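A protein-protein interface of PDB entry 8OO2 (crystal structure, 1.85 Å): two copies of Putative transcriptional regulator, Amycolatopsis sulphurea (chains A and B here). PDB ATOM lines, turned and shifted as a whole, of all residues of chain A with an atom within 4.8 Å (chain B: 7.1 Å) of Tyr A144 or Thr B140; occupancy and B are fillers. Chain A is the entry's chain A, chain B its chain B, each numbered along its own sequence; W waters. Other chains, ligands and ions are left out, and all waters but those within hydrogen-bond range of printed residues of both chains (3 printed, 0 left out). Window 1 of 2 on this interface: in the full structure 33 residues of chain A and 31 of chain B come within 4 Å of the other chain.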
ATOM      1  N   THR A 140       9.414  37.723 -15.152  1.00  0.00           N
ATOM      2  CA  THR A 140       8.940  36.331 -15.124  1.00  0.00           C
ATOM      3  C   THR A 140       8.817  35.825 -13.697  1.00  0.00           C
ATOM      4  O   THR A 140       7.793  35.217 -13.320  1.00  0.00           O
ATOM      5  CB  THR A 140       9.879  35.430 -15.915  1.00  0.00           C
ATOM      6  OG1 THR A 140       9.855  35.819 -17.267  1.00  0.00           O
ATOM      7  CG2 THR A 140       9.474  33.994 -15.767  1.00  0.00           C
ATOM      8  N   ILE A 141       9.821  36.092 -12.870  1.00  0.00           N
ATOM      9  CA  ILE A 141       9.778  35.600 -11.489  1.00  0.00           C
ATOM     10  C   ILE A 141       8.634  36.245 -10.741  1.00  0.00           C
ATOM     11  O   ILE A 141       7.923  35.578  -9.971  1.00  0.00           O
ATOM     12  CB  ILE A 141      11.123  35.854 -10.776  1.00  0.00           C
ATOM     13  CG1 ILE A 141      12.219  34.997 -11.354  1.00  0.00           C
ATOM     14  CG2 ILE A 141      10.986  35.625  -9.259  1.00  0.00           C
ATOM     15  CD1 ILE A 141      12.133  33.510 -11.057  1.00  0.00           C
ATOM     16  N   GLY A 142       8.414  37.547 -10.956  1.00  0.00           N
ATOM     17  CA  GLY A 142       7.326  38.233 -10.264  1.00  0.00           C
ATOM     18  C   GLY A 142       5.958  37.757 -10.758  1.00  0.00           C
ATOM     19  O   GLY A 142       5.015  37.671  -9.978  1.00  0.00           O
ATOM     20  N   ARG A 143       5.828  37.500 -12.040  1.00  0.00           N
ATOM     21  CA  ARG A 143       4.551  37.013 -12.583  1.00  0.00           C
ATOM     22  C   ARG A 143       4.269  35.597 -12.116  1.00  0.00           C
ATOM     23  O   ARG A 143       3.124  35.264 -11.848  1.00  0.00           O
ATOM     24  CB  ARG A 143       4.503  37.165 -14.084  1.00  0.00           C
ATOM     25  CG  ARG A 143       4.359  38.630 -14.497  1.00  0.00           C
ATOM     26  CD  ARG A 143       4.343  38.892 -15.954  1.00  0.00           C
ATOM     27  NE  ARG A 143       4.249  40.305 -16.194  1.00  0.00           N
ATOM     28  CZ  ARG A 143       4.389  40.940 -17.311  1.00  0.00           C
ATOM     29  NH1 ARG A 143       4.553  40.271 -18.468  1.00  0.00           N
ATOM     30  NH2 ARG A 143       4.352  42.279 -17.284  1.00  0.00           N
ATOM     31  N   TYR A 144       5.265  34.746 -12.042  1.00  0.00           N
ATOM     32  CA  TYR A 144       5.073  33.442 -11.463  1.00  0.00           C
ATOM     33  C   TYR A 144       4.546  33.591 -10.017  1.00  0.00           C
ATOM     34  O   TYR A 144       3.548  32.991  -9.638  1.00  0.00           O
ATOM     35  CB  TYR A 144       6.358  32.626 -11.468  1.00  0.00           C
ATOM     36  CG  TYR A 144       6.238  31.354 -10.668  1.00  0.00           C
ATOM     37  CD1 TYR A 144       5.471  30.285 -11.116  1.00  0.00           C
ATOM     38  CD2 TYR A 144       6.853  31.236  -9.400  1.00  0.00           C
ATOM     39  CE1 TYR A 144       5.305  29.143 -10.368  1.00  0.00           C
ATOM     40  CE2 TYR A 144       6.704  30.082  -8.659  1.00  0.00           C
ATOM     41  CZ  TYR A 144       5.925  29.050  -9.122  1.00  0.00           C
ATOM     42  OH  TYR A 144       5.768  27.884  -8.387  1.00  0.00           O
ATOM     43  N   THR A 145       5.217  34.405  -9.204  1.00  0.00           N
ATOM     44  CA  THR A 145       4.823  34.572  -7.818  1.00  0.00           C
ATOM     45  C   THR A 145       3.428  35.169  -7.740  1.00  0.00           C
ATOM     46  O   THR A 145       2.637  34.751  -6.919  1.00  0.00           O
ATOM     47  CB  THR A 145       5.816  35.481  -7.087  1.00  0.00           C
ATOM     48  OG1 THR A 145       7.165  34.940  -7.304  1.00  0.00           O
ATOM     49  CG2 THR A 145       5.561  35.491  -5.639  1.00  0.00           C
ATOM     50  N   LEU A 146       3.123  36.127  -8.629  1.00  0.00           N
ATOM     51  CA  LEU A 146       1.793  36.723  -8.642  1.00  0.00           C
ATOM     52  C   LEU A 146       0.731  35.672  -8.923  1.00  0.00           C
ATOM     53  O   LEU A 146      -0.333  35.671  -8.281  1.00  0.00           O
ATOM     54  CB  LEU A 146       1.716  37.831  -9.675  1.00  0.00           C
ATOM     55  CG  LEU A 146       0.391  38.567  -9.814  1.00  0.00           C
ATOM     56  CD1 LEU A 146       0.072  39.406  -8.605  1.00  0.00           C
ATOM     57  CD2 LEU A 146       0.435  39.465 -11.075  1.00  0.00           C
ATOM     58  N   GLY A 147       0.984  34.811  -9.895  1.00  0.00           N
ATOM     59  CA  GLY A 147       0.007  33.760 -10.201  1.00  0.00           C
ATOM     60  C   GLY A 147      -0.229  32.824  -9.038  1.00  0.00           C
ATOM     61  O   GLY A 147      -1.363  32.455  -8.746  1.00  0.00           O
ATOM     62  N   CYS A 148       0.835  32.455  -8.314  1.00  0.00           N
ATOM     63  CA  CYS A 148       0.670  31.608  -7.149  1.00  0.00           C
ATOM     64  C   CYS A 148      -0.161  32.311  -6.074  1.00  0.00           C
ATOM     65  O   CYS A 148      -1.128  31.775  -5.575  1.00  0.00           O
ATOM     66  CB  CYS A 148       1.996  31.181  -6.582  1.00  0.00           C
ATOM     67  SG  CYS A 148       2.981  30.125  -7.773  1.00  0.00           S
ATOM     68  N   THR A 169       3.938  23.755  -3.572  1.00  0.00           N
ATOM     69  CA  THR A 169       3.666  24.027  -4.960  1.00  0.00           C
ATOM     70  C   THR A 169       4.428  25.256  -5.427  1.00  0.00           C
ATOM     71  O   THR A 169       5.088  25.241  -6.487  1.00  0.00           O
ATOM     72  CB  THR A 169       2.148  24.222  -5.158  1.00  0.00           C
ATOM     73  OG1 THR A 169       1.461  22.986  -4.806  1.00  0.00           O
ATOM     74  CG2 THR A 169       1.846  24.522  -6.579  1.00  0.00           C
ATOM     75  N   PHE A 170       4.400  26.317  -4.640  1.00  0.00           N
ATOM     76  CA  PHE A 170       5.154  27.519  -5.013  1.00  0.00           C
ATOM     77  C   PHE A 170       6.636  27.227  -5.157  1.00  0.00           C
ATOM     78  O   PHE A 170       7.250  27.626  -6.147  1.00  0.00           O
ATOM     79  CB  PHE A 170       4.922  28.610  -4.008  1.00  0.00           C
ATOM     80  CG  PHE A 170       5.842  29.777  -4.121  1.00  0.00           C
ATOM     81  CD1 PHE A 170       5.659  30.704  -5.107  1.00  0.00           C
ATOM     82  CD2 PHE A 170       6.919  29.936  -3.239  1.00  0.00           C
ATOM     83  CE1 PHE A 170       6.523  31.796  -5.211  1.00  0.00           C
ATOM     84  CE2 PHE A 170       7.755  31.012  -3.324  1.00  0.00           C
ATOM     85  CZ  PHE A 170       7.583  31.952  -4.336  1.00  0.00           C
ATOM     86  N   GLU A 171       7.224  26.541  -4.183  1.00  0.00           N
ATOM     87  CA  GLU A 171       8.658  26.277  -4.212  1.00  0.00           C
ATOM     88  C   GLU A 171       9.025  25.338  -5.346  1.00  0.00           C
ATOM     89  O   GLU A 171      10.070  25.498  -5.994  1.00  0.00           O
ATOM     90  CB  GLU A 171       9.104  25.679  -2.876  1.00  0.00           C
ATOM     91  CG  GLU A 171       9.285  26.684  -1.774  1.00  0.00           C
ATOM     92  CD  GLU A 171      10.473  27.616  -2.007  1.00  0.00           C
ATOM     93  OE1 GLU A 171      11.449  27.201  -2.714  1.00  0.00           O
ATOM     94  OE2 GLU A 171      10.436  28.755  -1.498  1.00  0.00           O
ATOM     95  N   PHE A 172       8.168  24.357  -5.634  1.00  0.00           N
ATOM     96  CA  PHE A 172       8.424  23.457  -6.739  1.00  0.00           C
ATOM     97  C   PHE A 172       8.608  24.215  -8.035  1.00  0.00           C
ATOM     98  O   PHE A 172       9.576  23.990  -8.747  1.00  0.00           O
ATOM     99  CB  PHE A 172       7.271  22.442  -6.863  1.00  0.00           C
ATOM    100  CG  PHE A 172       7.442  21.460  -7.989  1.00  0.00           C
ATOM    101  CD1 PHE A 172       8.064  20.239  -7.759  1.00  0.00           C
ATOM    102  CD2 PHE A 172       6.957  21.739  -9.238  1.00  0.00           C
ATOM    103  CE1 PHE A 172       8.219  19.320  -8.788  1.00  0.00           C
ATOM    104  CE2 PHE A 172       7.079  20.800 -10.276  1.00  0.00           C
ATOM    105  CZ  PHE A 172       7.734  19.604 -10.041  1.00  0.00           C
ATOM    106  N   GLY A 173       7.669  25.086  -8.369  1.00  0.00           N
ATOM    107  CA  GLY A 173       7.784  25.858  -9.580  1.00  0.00           C
ATOM    108  C   GLY A 173       8.900  26.891  -9.551  1.00  0.00           C
ATOM    109  O   GLY A 173       9.572  27.112 -10.588  1.00  0.00           O
ATOM    110  N   LEU A 174       9.107  27.541  -8.392  1.00  0.00           N
ATOM    111  CA  LEU A 174      10.192  28.495  -8.288  1.00  0.00           C
ATOM    112  C   LEU A 174      11.528  27.816  -8.623  1.00  0.00           C
ATOM    113  O   LEU A 174      12.324  28.358  -9.397  1.00  0.00           O
ATOM    114  CB  LEU A 174      10.231  29.074  -6.875  1.00  0.00           C
ATOM    115  CG  LEU A 174      11.343  30.052  -6.569  1.00  0.00           C
ATOM    116  CD1 LEU A 174      11.269  31.239  -7.509  1.00  0.00           C
ATOM    117  CD2 LEU A 174      11.254  30.521  -5.102  1.00  0.00           C
ATOM    118  N   LEU A 177      11.802  26.900 -12.294  1.00  0.00           N
ATOM    119  CA  LEU A 177      12.005  28.083 -13.106  1.00  0.00           C
ATOM    120  C   LEU A 177      13.446  28.578 -12.971  1.00  0.00           C
ATOM    121  O   LEU A 177      14.101  28.898 -13.981  1.00  0.00           O
ATOM    122  CB  LEU A 177      11.030  29.177 -12.656  1.00  0.00           C
ATOM    123  CG  LEU A 177      11.023  30.517 -13.376  1.00  0.00           C
ATOM    124  CD1 LEU A 177      10.864  30.352 -14.879  1.00  0.00           C
ATOM    125  CD2 LEU A 177       9.840  31.369 -12.807  1.00  0.00           C
ATOM    126  N   ALA B 134       3.770  14.769 -10.934  1.00  0.00           N
ATOM    127  CA  ALA B 134       2.992  15.110 -12.117  1.00  0.00           C
ATOM    128  C   ALA B 134       1.879  16.098 -11.799  1.00  0.00           C
ATOM    129  O   ALA B 134       1.675  17.082 -12.524  1.00  0.00           O
ATOM    130  CB  ALA B 134       2.388  13.828 -12.721  1.00  0.00           C
ATOM    131  N   LEU B 135       1.173  15.893 -10.708  1.00  0.00           N
ATOM    132  CA  LEU B 135       0.132  16.845 -10.324  1.00  0.00           C
ATOM    133  C   LEU B 135       0.738  18.219  -9.994  1.00  0.00           C
ATOM    134  O   LEU B 135       0.223  19.276 -10.416  1.00  0.00           O
ATOM    135  CB  LEU B 135      -0.665  16.306  -9.149  1.00  0.00           C
ATOM    136  CG  LEU B 135      -1.758  17.193  -8.575  1.00  0.00           C
ATOM    137  CD1 LEU B 135      -2.757  17.579  -9.681  1.00  0.00           C
ATOM    138  CD2 LEU B 135      -2.444  16.523  -7.415  1.00  0.00           C
ATOM    139  N   THR B 136       1.822  18.236  -9.233  1.00  0.00           N
ATOM    140  CA  THR B 136       2.468  19.522  -8.918  1.00  0.00           C
ATOM    141  C   THR B 136       2.891  20.254 -10.194  1.00  0.00           C
ATOM    142  O   THR B 136       2.757  21.490 -10.298  1.00  0.00           O
ATOM    143  CB  THR B 136       3.656  19.290  -8.021  1.00  0.00           C
ATOM    144  OG1 THR B 136       3.262  18.506  -6.879  1.00  0.00           O
ATOM    145  CG2 THR B 136       4.213  20.625  -7.511  1.00  0.00           C
ATOM    146  N   VAL B 137       3.306  19.515 -11.216  1.00  0.00           N
ATOM    147  CA  VAL B 137       3.657  20.131 -12.488  1.00  0.00           C
ATOM    148  C   VAL B 137       2.448  20.805 -13.097  1.00  0.00           C
ATOM    149  O   VAL B 137       2.527  21.929 -13.598  1.00  0.00           O
ATOM    150  CB  VAL B 137       4.267  19.085 -13.456  1.00  0.00           C
ATOM    151  CG1 VAL B 137       4.323  19.661 -14.856  1.00  0.00           C
ATOM    152  CG2 VAL B 137       5.646  18.653 -12.980  1.00  0.00           C
ATOM    153  N   ILE B 138       1.327  20.112 -13.119  1.00  0.00           N
ATOM    154  CA  ILE B 138       0.090  20.674 -13.661  1.00  0.00           C
ATOM    155  C   ILE B 138      -0.267  21.976 -12.931  1.00  0.00           C
ATOM    156  O   ILE B 138      -0.536  22.997 -13.558  1.00  0.00           O
ATOM    157  CB  ILE B 138      -1.050  19.661 -13.553  1.00  0.00           C
ATOM    158  CG1 ILE B 138      -0.875  18.548 -14.594  1.00  0.00           C
ATOM    159  CG2 ILE B 138      -2.411  20.345 -13.695  1.00  0.00           C
ATOM    160  CD1 ILE B 138      -1.038  19.000 -16.067  1.00  0.00           C
ATOM    161  N   ILE B 139      -0.303  21.931 -11.603  1.00  0.00           N
ATOM    162  CA  ILE B 139      -0.717  23.103 -10.824  1.00  0.00           C
ATOM    163  C   ILE B 139       0.243  24.264 -11.107  1.00  0.00           C
ATOM    164  O   ILE B 139      -0.201  25.406 -11.345  1.00  0.00           O
ATOM    165  CB  ILE B 139      -0.762  22.777  -9.338  1.00  0.00           C
ATOM    166  CG1 ILE B 139      -1.777  21.687  -9.052  1.00  0.00           C
ATOM    167  CG2 ILE B 139      -1.047  24.036  -8.539  1.00  0.00           C
ATOM    168  CD1 ILE B 139      -1.685  21.099  -7.653  1.00  0.00           C
ATOM    169  N   THR B 140       1.556  23.977 -11.086  1.00  0.00           N
ATOM    170  CA  THR B 140       2.562  25.017 -11.310  1.00  0.00           C
ATOM    171  C   THR B 140       2.434  25.667 -12.688  1.00  0.00           C
ATOM    172  O   THR B 140       2.469  26.901 -12.814  1.00  0.00           O
ATOM    173  CB  THR B 140       3.973  24.411 -11.179  1.00  0.00           C
ATOM    174  OG1 THR B 140       4.183  24.065  -9.809  1.00  0.00           O
ATOM    175  CG2 THR B 140       5.010  25.394 -11.609  1.00  0.00           C
ATOM    176  N   ILE B 141       2.258  24.862 -13.737  1.00  0.00           N
ATOM    177  CA  ILE B 141       2.163  25.436 -15.085  1.00  0.00           C
ATOM    178  C   ILE B 141       0.920  26.328 -15.202  1.00  0.00           C
ATOM    179  O   ILE B 141       0.948  27.413 -15.821  1.00  0.00           O
ATOM    180  CB  ILE B 141       2.127  24.299 -16.135  1.00  0.00           C
ATOM    181  CG1 ILE B 141       3.483  23.627 -16.268  1.00  0.00           C
ATOM    182  CG2 ILE B 141       1.688  24.828 -17.499  1.00  0.00           C
ATOM    183  CD1 ILE B 141       4.505  24.440 -16.997  1.00  0.00           C
ATOM    184  N   GLY B 142      -0.182  25.927 -14.583  1.00  0.00           N
ATOM    185  CA  GLY B 142      -1.399  26.721 -14.668  1.00  0.00           C
ATOM    186  C   GLY B 142      -1.232  28.049 -13.913  1.00  0.00           C
ATOM    187  O   GLY B 142      -1.718  29.074 -14.356  1.00  0.00           O
ATOM    188  N   ARG B 143      -0.508  28.033 -12.808  1.00  0.00           N
ATOM    189  CA  ARG B 143      -0.333  29.224 -11.984  1.00  0.00           C
ATOM    190  C   ARG B 143       0.644  30.175 -12.628  1.00  0.00           C
ATOM    191  O   ARG B 143       0.434  31.377 -12.608  1.00  0.00           O
ATOM    192  CB  ARG B 143       0.089  28.831 -10.571  1.00  0.00           C
ATOM    193  CG  ARG B 143      -1.167  28.355  -9.743  1.00  0.00           C
ATOM    194  CD  ARG B 143      -0.835  27.874  -8.364  1.00  0.00           C
ATOM    195  NE  ARG B 143      -2.030  27.303  -7.775  1.00  0.00           N
ATOM    196  CZ  ARG B 143      -2.103  26.723  -6.594  1.00  0.00           C
ATOM    197  NH1 ARG B 143      -1.047  26.636  -5.799  1.00  0.00           N
ATOM    198  NH2 ARG B 143      -3.261  26.211  -6.199  1.00  0.00           N
ATOM    199  N   TYR B 144       1.721  29.666 -13.241  1.00  0.00           N
ATOM    200  CA  TYR B 144       2.571  30.539 -14.033  1.00  0.00           C
ATOM    201  C   TYR B 144       1.762  31.233 -15.130  1.00  0.00           C
ATOM    202  O   TYR B 144       1.816  32.455 -15.305  1.00  0.00           O
ATOM    203  CB  TYR B 144       3.709  29.745 -14.682  1.00  0.00           C
ATOM    204  CG  TYR B 144       4.447  30.561 -15.702  1.00  0.00           C
ATOM    205  CD1 TYR B 144       5.294  31.612 -15.318  1.00  0.00           C
ATOM    206  CD2 TYR B 144       4.306  30.329 -17.070  1.00  0.00           C
ATOM    207  CE1 TYR B 144       5.948  32.372 -16.263  1.00  0.00           C
ATOM    208  CE2 TYR B 144       4.971  31.075 -17.986  1.00  0.00           C
ATOM    209  CZ  TYR B 144       5.785  32.113 -17.577  1.00  0.00           C
ATOM    210  OH  TYR B 144       6.422  32.871 -18.489  1.00  0.00           O
ATOM    211  N   THR B 145       0.927  30.463 -15.835  1.00  0.00           N
ATOM    212  CA  THR B 145       0.156  31.068 -16.900  1.00  0.00           C
ATOM    213  C   THR B 145      -0.820  32.084 -16.353  1.00  0.00           C
ATOM    214  O   THR B 145      -1.014  33.157 -16.946  1.00  0.00           O
ATOM    215  CB  THR B 145      -0.594  29.963 -17.713  1.00  0.00           C
ATOM    216  OG1 THR B 145       0.386  29.019 -18.163  1.00  0.00           O
ATOM    217  CG2 THR B 145      -1.294  30.573 -18.865  1.00  0.00           C
ATOM    218  N   LEU B 146      -1.486  31.747 -15.252  1.00  0.00           N
ATOM    219  CA  LEU B 146      -2.448  32.657 -14.644  1.00  0.00           C
ATOM    220  C   LEU B 146      -1.766  33.967 -14.246  1.00  0.00           C
ATOM    221  O   LEU B 146      -2.327  35.064 -14.457  1.00  0.00           O
ATOM    222  CB  LEU B 146      -3.077  32.008 -13.413  1.00  0.00           C
ATOM    223  CG  LEU B 146      -4.081  32.854 -12.652  1.00  0.00           C
ATOM    224  CD1 LEU B 146      -5.353  33.079 -13.442  1.00  0.00           C
ATOM    225  CD2 LEU B 146      -4.402  32.183 -11.281  1.00  0.00           C
ATOM    226  N   GLY B 147      -0.558  33.870 -13.713  1.00  0.00           N
ATOM    227  CA  GLY B 147       0.145  35.084 -13.301  1.00  0.00           C
ATOM    228  C   GLY B 147       0.498  35.972 -14.491  1.00  0.00           C
ATOM    229  O   GLY B 147       0.370  37.191 -14.427  1.00  0.00           O
ATOM    230  N   CYS B 148       0.878  35.361 -15.612  1.00  0.00           N
ATOM    231  CA  CYS B 148       1.187  36.139 -16.803  1.00  0.00           C
ATOM    232  C   CYS B 148      -0.053  36.818 -17.325  1.00  0.00           C
ATOM    233  O   CYS B 148      -0.043  38.007 -17.636  1.00  0.00           O
ATOM    234  CB  CYS B 148       1.808  35.236 -17.869  1.00  0.00           C
ATOM    235  SG  CYS B 148       3.468  34.643 -17.349  1.00  0.00           S
ATOM    236  N   LEU B 177      10.710  27.215 -17.199  1.00  0.00           N
ATOM    237  CA  LEU B 177      10.008  26.294 -16.324  1.00  0.00           C
ATOM    238  C   LEU B 177      10.092  24.873 -16.864  1.00  0.00           C
ATOM    239  O   LEU B 177      10.453  23.939 -16.147  1.00  0.00           O
ATOM    240  CB  LEU B 177       8.555  26.740 -16.175  1.00  0.00           C
ATOM    241  CG  LEU B 177       7.705  26.055 -15.153  1.00  0.00           C
ATOM    242  CD1 LEU B 177       8.314  26.100 -13.772  1.00  0.00           C
ATOM    243  CD2 LEU B 177       6.300  26.747 -15.120  1.00  0.00           C
ATOM    244  N   LEU B 181      11.879  21.504 -15.227  1.00  0.00           N
ATOM    245  CA  LEU B 181      11.178  20.249 -14.970  1.00  0.00           C
ATOM    246  C   LEU B 181      11.885  19.086 -15.655  1.00  0.00           C
ATOM    247  O   LEU B 181      12.030  17.999 -15.077  1.00  0.00           O
ATOM    248  CB  LEU B 181       9.727  20.368 -15.450  1.00  0.00           C
ATOM    249  CG  LEU B 181       8.893  21.452 -14.796  1.00  0.00           C
ATOM    250  CD1 LEU B 181       7.554  21.577 -15.553  1.00  0.00           C
ATOM    251  CD2 LEU B 181       8.676  21.144 -13.322  1.00  0.00           C
HETATM  252  O   HOH W   1       4.976  37.478 -18.883  1.00  0.00           O
HETATM  253  O   HOH W   2       6.796  35.657 -17.821  1.00  0.00           O
HETATM  254  O   HOH W   3       3.295  26.724  -8.459  1.00  0.00           O
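Water W3 lies within hydrogen-bond range of OH of Tyr A144 (2.7 Å), O of Thr A169 (3.1 Å), OG1 of Thr B140 (3.1 Å) and SG of Cys A148 (3.5 Å). Water W1 bridges the guanidinium group of Arg A143 (2.9 Å) and the side-chain sulfur of Cys B148 (3.6 Å). Water W2 lies within hydrogen-bond range of OH of Tyr B144 (2.9 Å), OG1 of Thr A140 (3.1 Å) and SG of Cys B148 (3.5 Å).
The side-chain hydroxyl (OH) of Tyr A144 lies within hydrogen-bond range of the backbone NH (N) of Leu A174, at 3.4 Å. OH of Tyr A144 lies within hydrogen-bond range of O of Thr A169 (3.3 Å). O of Thr B136 sits at hydrogen-bond distance from OG1 of Thr B140. The side-chain hydroxyl (OH) of Tyr A144 lies close to the backbone NH (N) of Gly A173 (3.4 Å). O of Tyr A144 sits close to SG of Cys A148, at 3.5 Å. The side-chain hydroxyl (OH) of Tyr A144 sits at hydrogen-bond distance from the backbone carbonyl oxygen (O) of Phe A170, at 2.7 Å.
Hydrophobic or aromatic side chains of chain B within 4 Å of the printed part of chain A: Val B137, Ile B139, Tyr B144, Leu B146, Leu B177 and Leu B181. Hydrophobic or aromatic side chains of chain A that line the printed part of chain B: Tyr A144, Phe A172 and Leu A177. Among the printed residues, no Asp or Glu carboxylate lies within 4 Å of a Lys or Arg side-chain nitrogen of the other chain.
Tyr B144 touches Thr A140. Tyr A144 touches Thr B140 (CE1 to CG2, 3.96 Å). CA of Gly A147 touches CA of Gly B147, at 3.4 Å. Thr A169 touches Thr B140 (O to OG1, 3.6 Å). Thr B136 touches Phe A172 (CG2 to CG, 3.4 Å). Val B137 touches Phe A172 (CG2 to CZ, 3.7 Å). Thr B140 touches Phe A172 (OG1 to CD2, 3.7 Å). CG2 of Thr B140 touches CA of Gly A173, at 3.5 Å. CD1 of Leu B177 touches O of Gly A173 (3.6 Å). N of Leu A177 touches CD1 of Leu B177 (3.9 Å).
Of the printed residues of chain B, Tyr A144 touches Thr B140. Thr B140 touches just these residues of chain A: Tyr A144, Thr A169, Phe A172 and Gly A173. Printed residues of chain B within 4 Å of Arg A143: Gly B147 (3.3 Å). Of the printed residues of chain A, Arg B143 touches Gly A147 and Thr A169. Printed residues of chain A within 4 Å of Gly B147: Arg A143 and Gly A147. Of the printed residues of chain A, Val B137 touches Phe A172 (3.7 Å). Printed residues of chain A within 4 Å of Thr B136: Phe A172.
Arg A143 touches Gly B147, and with the chains exchanged Gly A147 touches Arg B143. Gly A147 touches Leu B146, but with the chains exchanged Leu A146 does not touch Gly B147 (4.1 Å). Gly B147 touches its own counterpart, Gly A147. Leu B177 touches its own counterpart, Leu A177. 10 positions are printed for both chains. Of the 16 pairs that touch across the chains among the printed residues, 6 have their exchanged pair printed and touching as well.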
